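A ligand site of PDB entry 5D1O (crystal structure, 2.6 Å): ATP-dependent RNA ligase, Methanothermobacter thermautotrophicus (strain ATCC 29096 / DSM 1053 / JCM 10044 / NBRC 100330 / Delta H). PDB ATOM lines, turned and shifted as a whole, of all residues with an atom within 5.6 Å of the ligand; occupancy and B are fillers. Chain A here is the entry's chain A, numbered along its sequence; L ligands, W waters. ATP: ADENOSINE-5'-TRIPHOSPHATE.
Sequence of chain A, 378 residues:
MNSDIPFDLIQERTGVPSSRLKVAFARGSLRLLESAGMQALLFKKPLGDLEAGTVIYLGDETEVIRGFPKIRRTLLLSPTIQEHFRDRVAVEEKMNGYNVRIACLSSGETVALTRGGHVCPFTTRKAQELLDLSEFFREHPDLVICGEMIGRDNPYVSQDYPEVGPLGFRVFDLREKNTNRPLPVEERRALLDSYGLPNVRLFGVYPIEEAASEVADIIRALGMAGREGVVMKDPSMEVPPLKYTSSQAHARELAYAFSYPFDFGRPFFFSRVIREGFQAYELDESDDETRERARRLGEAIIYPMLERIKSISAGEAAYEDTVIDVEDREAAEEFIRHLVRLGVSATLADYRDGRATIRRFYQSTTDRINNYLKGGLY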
ATOM      1  N   PHE A  68     -13.195 -25.013  16.009  1.00  0.00           N
ATOM      2  CA  PHE A  68     -13.474 -23.703  15.480  1.00  0.00           C
ATOM      3  C   PHE A  68     -13.010 -23.637  14.041  1.00  0.00           C
ATOM      4  O   PHE A  68     -11.870 -23.971  13.752  1.00  0.00           O
ATOM      5  CB  PHE A  68     -12.824 -22.600  16.300  1.00  0.00           C
ATOM      6  CG  PHE A  68     -13.384 -21.242  16.023  1.00  0.00           C
ATOM      7  CD1 PHE A  68     -14.640 -20.897  16.492  1.00  0.00           C
ATOM      8  CD2 PHE A  68     -12.694 -20.322  15.248  1.00  0.00           C
ATOM      9  CE1 PHE A  68     -15.187 -19.660  16.212  1.00  0.00           C
ATOM     10  CE2 PHE A  68     -13.240 -19.073  14.961  1.00  0.00           C
ATOM     11  CZ  PHE A  68     -14.473 -18.742  15.436  1.00  0.00           C
ATOM     12  N   PRO A  69     -13.924 -23.235  13.137  1.00  0.00           N
ATOM     13  CA  PRO A  69     -13.771 -23.093  11.677  1.00  0.00           C
ATOM     14  C   PRO A  69     -12.701 -22.090  11.240  1.00  0.00           C
ATOM     15  O   PRO A  69     -12.594 -21.000  11.795  1.00  0.00           O
ATOM     16  CB  PRO A  69     -15.146 -22.602  11.225  1.00  0.00           C
ATOM     17  CG  PRO A  69     -16.056 -23.039  12.282  1.00  0.00           C
ATOM     18  CD  PRO A  69     -15.308 -22.961  13.549  1.00  0.00           C
ATOM     19  N   LYS A  70     -11.928 -22.491  10.241  1.00  0.00           N
ATOM     20  CA  LYS A  70     -10.948 -21.609   9.624  1.00  0.00           C
ATOM     21  C   LYS A  70     -11.661 -20.384   9.057  1.00  0.00           C
ATOM     22  O   LYS A  70     -12.625 -20.521   8.321  1.00  0.00           O
ATOM     23  CB  LYS A  70     -10.166 -22.352   8.533  1.00  0.00           C
ATOM     24  CG  LYS A  70      -9.201 -23.397   9.088  1.00  0.00           C
ATOM     25  CD  LYS A  70      -8.121 -23.808   8.083  1.00  0.00           C
ATOM     26  CE  LYS A  70      -7.042 -24.655   8.773  1.00  0.00           C
ATOM     27  NZ  LYS A  70      -5.799 -24.823   7.949  1.00  0.00           N
ATOM     28  N   ILE A  71     -11.207 -19.196   9.432  1.00  0.00           N
ATOM     29  CA  ILE A  71     -11.773 -17.963   8.895  1.00  0.00           C
ATOM     30  C   ILE A  71     -10.899 -17.563   7.730  1.00  0.00           C
ATOM     31  O   ILE A  71      -9.671 -17.496   7.875  1.00  0.00           O
ATOM     32  CB  ILE A  71     -11.813 -16.815   9.919  1.00  0.00           C
ATOM     33  CG1 ILE A  71     -12.757 -17.153  11.075  1.00  0.00           C
ATOM     34  CG2 ILE A  71     -12.292 -15.549   9.284  1.00  0.00           C
ATOM     35  CD1 ILE A  71     -12.841 -16.060  12.142  1.00  0.00           C
ATOM     36  N   ARG A  72     -11.526 -17.328   6.576  1.00  0.00           N
ATOM     37  CA  ARG A  72     -10.778 -16.982   5.385  1.00  0.00           C
ATOM     38  C   ARG A  72     -10.240 -15.568   5.466  1.00  0.00           C
ATOM     39  O   ARG A  72     -10.731 -14.747   6.226  1.00  0.00           O
ATOM     40  CB  ARG A  72     -11.643 -17.165   4.136  1.00  0.00           C
ATOM     41  CG  ARG A  72     -11.876 -18.644   3.772  1.00  0.00           C
ATOM     42  CD  ARG A  72     -10.621 -19.343   3.186  1.00  0.00           C
ATOM     43  NE  ARG A  72     -10.308 -18.922   1.804  1.00  0.00           N
ATOM     44  CZ  ARG A  72     -10.411 -19.707   0.730  1.00  0.00           C
ATOM     45  NH1 ARG A  72     -10.804 -20.966   0.856  1.00  0.00           N
ATOM     46  NH2 ARG A  72     -10.111 -19.239  -0.468  1.00  0.00           N
ATOM     47  N   ARG A  73      -9.202 -15.292   4.681  1.00  0.00           N
ATOM     48  CA  ARG A  73      -8.529 -14.005   4.699  1.00  0.00           C
ATOM     49  C   ARG A  73      -8.766 -13.273   3.387  1.00  0.00           C
ATOM     50  O   ARG A  73      -8.905 -13.894   2.334  1.00  0.00           O
ATOM     51  CB  ARG A  73      -7.025 -14.204   4.925  1.00  0.00           C
ATOM     52  CG  ARG A  73      -6.228 -12.925   5.000  1.00  0.00           C
ATOM     53  CD  ARG A  73      -4.796 -13.188   5.423  1.00  0.00           C
ATOM     54  NE  ARG A  73      -4.675 -13.610   6.814  1.00  0.00           N
ATOM     55  CZ  ARG A  73      -4.480 -12.793   7.836  1.00  0.00           C
ATOM     56  NH1 ARG A  73      -4.389 -11.495   7.631  1.00  0.00           N
ATOM     57  NH2 ARG A  73      -4.377 -13.274   9.064  1.00  0.00           N
ATOM     58  N   GLU A  92     -16.164  -6.612  13.760  1.00  0.00           N
ATOM     59  CA  GLU A  92     -15.671  -6.734  15.140  1.00  0.00           C
ATOM     60  C   GLU A  92     -14.161  -6.562  15.176  1.00  0.00           C
ATOM     61  O   GLU A  92     -13.510  -6.589  14.133  1.00  0.00           O
ATOM     62  CB  GLU A  92     -16.036  -8.089  15.749  1.00  0.00           C
ATOM     63  CG  GLU A  92     -17.416  -8.583  15.392  1.00  0.00           C
ATOM     64  CD  GLU A  92     -17.750  -9.915  16.034  1.00  0.00           C
ATOM     65  OE1 GLU A  92     -16.925 -10.851  15.890  1.00  0.00           O
ATOM     66  OE2 GLU A  92     -18.804 -10.010  16.706  1.00  0.00           O
ATOM     67  N   GLU A  93     -13.601  -6.411  16.362  1.00  0.00           N
ATOM     68  CA  GLU A  93     -12.152  -6.331  16.492  1.00  0.00           C
ATOM     69  C   GLU A  93     -11.504  -7.703  16.565  1.00  0.00           C
ATOM     70  O   GLU A  93     -11.929  -8.564  17.326  1.00  0.00           O
ATOM     71  CB  GLU A  93     -11.759  -5.527  17.727  1.00  0.00           C
ATOM     72  CG  GLU A  93     -10.294  -5.630  18.029  1.00  0.00           C
ATOM     73  CD  GLU A  93      -9.869  -4.640  19.070  1.00  0.00           C
ATOM     74  OE1 GLU A  93      -8.696  -4.647  19.483  1.00  0.00           O
ATOM     75  OE2 GLU A  93     -10.736  -3.831  19.475  1.00  0.00           O
ATOM     76  N   LYS A  94     -10.470  -7.870  15.768  1.00  0.00           N
ATOM     77  CA  LYS A  94      -9.649  -9.066  15.829  1.00  0.00           C
ATOM     78  C   LYS A  94      -8.751  -8.998  17.044  1.00  0.00           C
ATOM     79  O   LYS A  94      -7.875  -8.134  17.140  1.00  0.00           O
ATOM     80  CB  LYS A  94      -8.818  -9.199  14.567  1.00  0.00           C
ATOM     81  CG  LYS A  94      -8.400 -10.587  14.261  1.00  0.00           C
ATOM     82  CD  LYS A  94      -7.940 -10.662  12.842  1.00  0.00           C
ATOM     83  CE  LYS A  94      -7.576 -12.071  12.503  1.00  0.00           C
ATOM     84  NZ  LYS A  94      -6.555 -12.554  13.463  1.00  0.00           N
ATOM     85  N   MET A  95      -8.969  -9.914  17.981  1.00  0.00           N
ATOM     86  CA  MET A  95      -8.188  -9.983  19.212  1.00  0.00           C
ATOM     87  C   MET A  95      -6.977 -10.900  19.050  1.00  0.00           C
ATOM     88  O   MET A  95      -7.116 -12.091  18.776  1.00  0.00           O
ATOM     89  CB  MET A  95      -9.053 -10.448  20.391  1.00  0.00           C
ATOM     90  CG  MET A  95     -10.221  -9.518  20.707  1.00  0.00           C
ATOM     91  SD  MET A  95      -9.705  -7.803  20.939  1.00  0.00           S
ATOM     92  CE  MET A  95      -9.036  -7.826  22.605  1.00  0.00           C
ATOM     93  N   ASN A  96      -5.787 -10.348  19.236  1.00  0.00           N
ATOM     94  CA  ASN A  96      -4.586 -11.153  19.166  1.00  0.00           C
ATOM     95  C   ASN A  96      -4.366 -11.967  20.424  1.00  0.00           C
ATOM     96  O   ASN A  96      -3.868 -11.428  21.401  1.00  0.00           O
ATOM     97  CB  ASN A  96      -3.373 -10.267  18.920  1.00  0.00           C
ATOM     98  CG  ASN A  96      -2.110 -11.052  18.819  1.00  0.00           C
ATOM     99  OD1 ASN A  96      -2.122 -12.209  18.392  1.00  0.00           O
ATOM    100  ND2 ASN A  96      -1.009 -10.455  19.224  1.00  0.00           N
ATOM    101  N   TYR A  98      -5.334 -16.320  22.094  1.00  0.00           N
ATOM    102  CA  TYR A  98      -5.472 -17.691  21.639  1.00  0.00           C
ATOM    103  C   TYR A  98      -6.901 -18.193  21.807  1.00  0.00           C
ATOM    104  O   TYR A  98      -7.544 -18.008  22.847  1.00  0.00           O
ATOM    105  CB  TYR A  98      -4.463 -18.616  22.326  1.00  0.00           C
ATOM    106  CG  TYR A  98      -4.709 -18.809  23.770  1.00  0.00           C
ATOM    107  CD1 TYR A  98      -4.239 -17.877  24.703  1.00  0.00           C
ATOM    108  CD2 TYR A  98      -5.420 -19.904  24.233  1.00  0.00           C
ATOM    109  CE1 TYR A  98      -4.474 -18.071  26.070  1.00  0.00           C
ATOM    110  CE2 TYR A  98      -5.659 -20.094  25.591  1.00  0.00           C
ATOM    111  CZ  TYR A  98      -5.193 -19.166  26.501  1.00  0.00           C
ATOM    112  OH  TYR A  98      -5.449 -19.353  27.832  1.00  0.00           O
ATOM    113  N   ASN A  99      -7.352 -18.814  20.721  1.00  0.00           N
ATOM    114  CA  ASN A  99      -8.666 -19.396  20.556  1.00  0.00           C
ATOM    115  C   ASN A  99      -9.051 -20.332  21.672  1.00  0.00           C
ATOM    116  O   ASN A  99      -8.314 -21.245  22.013  1.00  0.00           O
ATOM    117  CB  ASN A  99      -8.732 -20.133  19.222  1.00  0.00           C
ATOM    118  CG  ASN A  99     -10.156 -20.362  18.758  1.00  0.00           C
ATOM    119  OD1 ASN A  99     -11.040 -20.654  19.558  1.00  0.00           O
ATOM    120  ND2 ASN A  99     -10.380 -20.204  17.460  1.00  0.00           N
ATOM    121  N   ARG A 115      -7.118 -24.670  20.493  1.00  0.00           N
ATOM    122  CA  ARG A 115      -7.588 -24.876  19.130  1.00  0.00           C
ATOM    123  C   ARG A 115      -7.490 -26.324  18.660  1.00  0.00           C
ATOM    124  O   ARG A 115      -8.320 -26.786  17.877  1.00  0.00           O
ATOM    125  CB  ARG A 115      -6.836 -23.981  18.158  1.00  0.00           C
ATOM    126  CG  ARG A 115      -7.478 -23.897  16.784  1.00  0.00           C
ATOM    127  CD  ARG A 115      -8.831 -23.166  16.819  1.00  0.00           C
ATOM    128  NE  ARG A 115      -9.497 -23.140  15.501  1.00  0.00           N
ATOM    129  CZ  ARG A 115      -9.097 -22.394  14.482  1.00  0.00           C
ATOM    130  NH1 ARG A 115      -8.025 -21.608  14.617  1.00  0.00           N
ATOM    131  NH2 ARG A 115      -9.754 -22.408  13.334  1.00  0.00           N
ATOM    132  N   GLY A 147     -14.030 -17.775  22.190  1.00  0.00           N
ATOM    133  CA  GLY A 147     -13.420 -16.507  22.505  1.00  0.00           C
ATOM    134  C   GLY A 147     -11.923 -16.374  22.277  1.00  0.00           C
ATOM    135  O   GLY A 147     -11.263 -17.277  21.746  1.00  0.00           O
ATOM    136  N   GLU A 148     -11.385 -15.231  22.652  1.00  0.00           N
ATOM    137  CA  GLU A 148      -9.967 -15.026  22.603  1.00  0.00           C
ATOM    138  C   GLU A 148      -9.427 -14.678  23.987  1.00  0.00           C
ATOM    139  O   GLU A 148      -9.773 -13.651  24.559  1.00  0.00           O
ATOM    140  CB  GLU A 148      -9.632 -13.919  21.616  1.00  0.00           C
ATOM    141  CG  GLU A 148      -8.225 -14.022  21.043  1.00  0.00           C
ATOM    142  CD  GLU A 148      -8.115 -15.073  19.935  1.00  0.00           C
ATOM    143  OE1 GLU A 148      -9.101 -15.775  19.631  1.00  0.00           O
ATOM    144  OE2 GLU A 148      -7.010 -15.190  19.369  1.00  0.00           O
ATOM    145  N   PHE A 172     -16.396 -14.154  20.872  1.00  0.00           N
ATOM    146  CA  PHE A 172     -16.765 -13.728  19.540  1.00  0.00           C
ATOM    147  C   PHE A 172     -17.737 -14.699  18.899  1.00  0.00           C
ATOM    148  O   PHE A 172     -18.099 -14.524  17.747  1.00  0.00           O
ATOM    149  CB  PHE A 172     -15.518 -13.573  18.648  1.00  0.00           C
ATOM    150  CG  PHE A 172     -14.551 -14.720  18.710  1.00  0.00           C
ATOM    151  CD1 PHE A 172     -14.871 -15.954  18.166  1.00  0.00           C
ATOM    152  CD2 PHE A 172     -13.309 -14.556  19.279  1.00  0.00           C
ATOM    153  CE1 PHE A 172     -13.972 -17.006  18.221  1.00  0.00           C
ATOM    154  CE2 PHE A 172     -12.387 -15.609  19.334  1.00  0.00           C
ATOM    155  CZ  PHE A 172     -12.718 -16.840  18.808  1.00  0.00           C
ATOM    156  N   VAL A 200     -16.348  -9.336  22.392  1.00  0.00           N
ATOM    157  CA  VAL A 200     -15.351  -8.619  21.592  1.00  0.00           C
ATOM    158  C   VAL A 200     -15.945  -7.325  21.109  1.00  0.00           C
ATOM    159  O   VAL A 200     -17.117  -7.299  20.764  1.00  0.00           O
ATOM    160  CB  VAL A 200     -14.875  -9.409  20.349  1.00  0.00           C
ATOM    161  CG1 VAL A 200     -13.770 -10.399  20.683  1.00  0.00           C
ATOM    162  CG2 VAL A 200     -16.060 -10.073  19.663  1.00  0.00           C
ATOM    163  N   GLU A 228      -4.444  -5.645  16.301  1.00  0.00           N
ATOM    164  CA  GLU A 228      -4.190  -6.625  15.255  1.00  0.00           C
ATOM    165  C   GLU A 228      -5.047  -6.380  14.033  1.00  0.00           C
ATOM    166  O   GLU A 228      -4.555  -6.455  12.911  1.00  0.00           O
ATOM    167  CB  GLU A 228      -4.417  -8.052  15.752  1.00  0.00           C
ATOM    168  CG  GLU A 228      -3.859  -9.094  14.784  1.00  0.00           C
ATOM    169  CD  GLU A 228      -4.417 -10.494  15.009  1.00  0.00           C
ATOM    170  OE1 GLU A 228      -5.345 -10.620  15.835  1.00  0.00           O
ATOM    171  OE2 GLU A 228      -3.951 -11.464  14.358  1.00  0.00           O
ATOM    172  N   VAL A 231     -12.370  -8.530  12.168  1.00  0.00           N
ATOM    173  CA  VAL A 231     -13.058  -9.715  11.665  1.00  0.00           C
ATOM    174  C   VAL A 231     -14.442  -9.294  11.185  1.00  0.00           C
ATOM    175  O   VAL A 231     -15.227  -8.765  11.937  1.00  0.00           O
ATOM    176  CB  VAL A 231     -13.228 -10.815  12.746  1.00  0.00           C
ATOM    177  CG1 VAL A 231     -14.299 -11.827  12.325  1.00  0.00           C
ATOM    178  CG2 VAL A 231     -11.905 -11.481  13.068  1.00  0.00           C
ATOM    179  N   LYS A 233     -18.245  -9.964   9.577  1.00  0.00           N
ATOM    180  CA  LYS A 233     -19.244 -11.041   9.705  1.00  0.00           C
ATOM    181  C   LYS A 233     -20.579 -10.732   9.041  1.00  0.00           C
ATOM    182  O   LYS A 233     -21.088  -9.602   9.054  1.00  0.00           O
ATOM    183  CB  LYS A 233     -19.463 -11.396  11.193  1.00  0.00           C
ATOM    184  CG  LYS A 233     -18.179 -11.819  11.924  1.00  0.00           C
ATOM    185  CD  LYS A 233     -18.456 -12.335  13.340  1.00  0.00           C
ATOM    186  CE  LYS A 233     -17.256 -13.136  13.898  1.00  0.00           C
ATOM    187  NZ  LYS A 233     -17.609 -14.315  14.728  1.00  0.00           N
ATOM    188  N   LYS A 243     -11.330 -12.338   7.684  1.00  0.00           N
ATOM    189  CA  LYS A 243     -10.389 -11.589   8.524  1.00  0.00           C
ATOM    190  C   LYS A 243      -9.461 -10.732   7.668  1.00  0.00           C
ATOM    191  O   LYS A 243      -9.152 -11.066   6.536  1.00  0.00           O
ATOM    192  CB  LYS A 243      -9.575 -12.545   9.410  1.00  0.00           C
ATOM    193  CG  LYS A 243      -8.964 -13.706   8.650  1.00  0.00           C
ATOM    194  CD  LYS A 243      -8.059 -14.557   9.517  1.00  0.00           C
ATOM    195  CE  LYS A 243      -7.340 -15.592   8.656  1.00  0.00           C
ATOM    196  NZ  LYS A 243      -6.600 -16.607   9.464  1.00  0.00           N
ATOM    197  N   GLU A 253       4.112  -9.499  13.875  1.00  0.00           N
ATOM    198  CA  GLU A 253       4.342 -10.910  13.660  1.00  0.00           C
ATOM    199  C   GLU A 253       5.684 -11.150  13.030  1.00  0.00           C
ATOM    200  O   GLU A 253       6.436 -12.030  13.451  1.00  0.00           O
ATOM    201  CB  GLU A 253       3.265 -11.503  12.752  1.00  0.00           C
ATOM    202  CG  GLU A 253       1.934 -11.652  13.398  1.00  0.00           C
ATOM    203  CD  GLU A 253       0.929 -12.204  12.440  1.00  0.00           C
ATOM    204  OE1 GLU A 253       1.291 -12.333  11.247  1.00  0.00           O
ATOM    205  OE2 GLU A 253      -0.223 -12.484  12.881  1.00  0.00           O
HETATM  206  PG  ATP L   1      -7.579 -19.898  11.047  1.00  0.00           P
HETATM  207  O1G ATP L   1      -6.513 -19.874   9.975  1.00  0.00           O
HETATM  208  O2G ATP L   1      -8.813 -19.094  10.722  1.00  0.00           O
HETATM  209  O3G ATP L   1      -7.861 -21.294  11.537  1.00  0.00           O
HETATM  210  PB  ATP L   1      -5.555 -18.320  12.433  1.00  0.00           P
HETATM  211  O1B ATP L   1      -5.092 -17.919  11.043  1.00  0.00           O
HETATM  212  O2B ATP L   1      -4.626 -19.055  13.403  1.00  0.00           O
HETATM  213  O3B ATP L   1      -6.964 -19.144  12.344  1.00  0.00           O
HETATM  214  PA  ATP L   1      -5.657 -15.472  12.935  1.00  0.00           P
HETATM  215  O1A ATP L   1      -5.285 -15.297  11.482  1.00  0.00           O
HETATM  216  O2A ATP L   1      -4.728 -14.911  13.982  1.00  0.00           O
HETATM  217  O3A ATP L   1      -5.997 -17.015  13.289  1.00  0.00           O
HETATM  218  O5' ATP L   1      -7.153 -14.921  13.146  1.00  0.00           O
HETATM  219  C5' ATP L   1      -8.309 -15.763  13.049  1.00  0.00           C
HETATM  220  C4' ATP L   1      -8.606 -16.126  14.498  1.00  0.00           C
HETATM  221  O4' ATP L   1      -8.674 -14.917  15.251  1.00  0.00           O
HETATM  222  C3' ATP L   1      -9.885 -16.893  14.783  1.00  0.00           C
HETATM  223  O3' ATP L   1      -9.738 -18.305  14.558  1.00  0.00           O
HETATM  224  C2' ATP L   1     -10.064 -16.537  16.236  1.00  0.00           C
HETATM  225  O2' ATP L   1      -9.337 -17.483  17.022  1.00  0.00           O
HETATM  226  C1' ATP L   1      -9.377 -15.183  16.446  1.00  0.00           C
HETATM  227  N9  ATP L   1     -10.291 -14.012  16.622  1.00  0.00           N
HETATM  228  C8  ATP L   1      -9.969 -12.906  17.322  1.00  0.00           C
HETATM  229  N7  ATP L   1     -10.985 -12.000  17.327  1.00  0.00           N
HETATM  230  C5  ATP L   1     -11.992 -12.546  16.613  1.00  0.00           C
HETATM  231  C6  ATP L   1     -13.350 -12.132  16.213  1.00  0.00           C
HETATM  232  N6  ATP L   1     -13.856 -10.933  16.593  1.00  0.00           N
HETATM  233  N1  ATP L   1     -14.080 -12.992  15.474  1.00  0.00           N
HETATM  234  C2  ATP L   1     -13.591 -14.185  15.104  1.00  0.00           C
HETATM  235  N3  ATP L   1     -12.361 -14.627  15.419  1.00  0.00           N
HETATM  236  C4  ATP L   1     -11.530 -13.867  16.161  1.00  0.00           C
HETATM  237  O   HOH W   1      -2.888 -16.937  15.550  1.00  0.00           O
HETATM  238  O   HOH W   2      -3.305 -14.655  17.150  1.00  0.00           O
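Residues that only touch the ligand: Val 231 (3.4 Å), Lys 70 (3.5 Å), Phe 172 (3.5 Å), Lys 233 (3.5 Å), Glu 228 (3.6 Å), Phe 68 (3.6 Å) and Val 200 (3.9 Å).
The nearest printed residue that does not touch the ligand is Pro 69 (4.4 Å).
Water W2 bridges OD1 of Asn 96 (3.0 Å) and O2A of the ligand (3.5 Å).
The side-chain carboxylate of Glu 148 is in hydrogen-bond range of an oxygen (O2') of the ligand (3.1 Å).
The backbone carbonyl oxygen (O) of Glu 93 lies within hydrogen-bond range of a nitrogen (N6) of the ligand (3.1 Å).
O1B of the ligand is in salt-bridge range of NZ of Lys 243 (2.5 Å).
An oxygen (O3G) of the ligand lies within salt-bridge range of the guanidinium group (NH2) of Arg 115, 2.8 Å away.
O2' of the ligand sits at hydrogen-bond distance from ND2 of Asn 99.
N of Met 95 lies within hydrogen-bond range of N7 of the ligand, 3.0 Å away.
The backbone NH (N) of Ile 71 is in hydrogen-bond range of an oxygen (O2G) of the ligand.
The side-chain amino group of Lys 94 lies within salt-bridge range of an oxygen (O2A) of the ligand, at 3.0 Å.
The side-chain carboxylate of Glu 92 lies within hydrogen-bond range of a nitrogen (N6) of the ligand (3.1 Å).
The guanidinium group of Arg 73 is in salt-bridge range of an oxygen (O1A) of the ligand, 3.3 Å away.
O of Phe 172 sits at hydrogen-bond distance from NZ of Lys 233 (3.1 Å).
N of Glu 92 is in hydrogen-bond range of O of Val 231, at 3.0 Å.
The side-chain amino group of Lys 94 is in salt-bridge range of the side-chain carboxylate of Glu 228, at 3.0 Å.
OE1 of Glu 228 sits at hydrogen-bond distance from N of Asn 96 (3.4 Å).
NZ of Lys 233 is in salt-bridge range of OE1 of Glu 92 (3.7 Å).
NH2 of Arg 115 lies within hydrogen-bond range of O of Phe 68 (2.7 Å).
N of Tyr 98 lies within hydrogen-bond range of OE2 of Glu 148 (3.4 Å).
The backbone carbonyl oxygen (O) of Arg 72 sits at hydrogen-bond distance from the backbone NH (N) of Lys 243.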
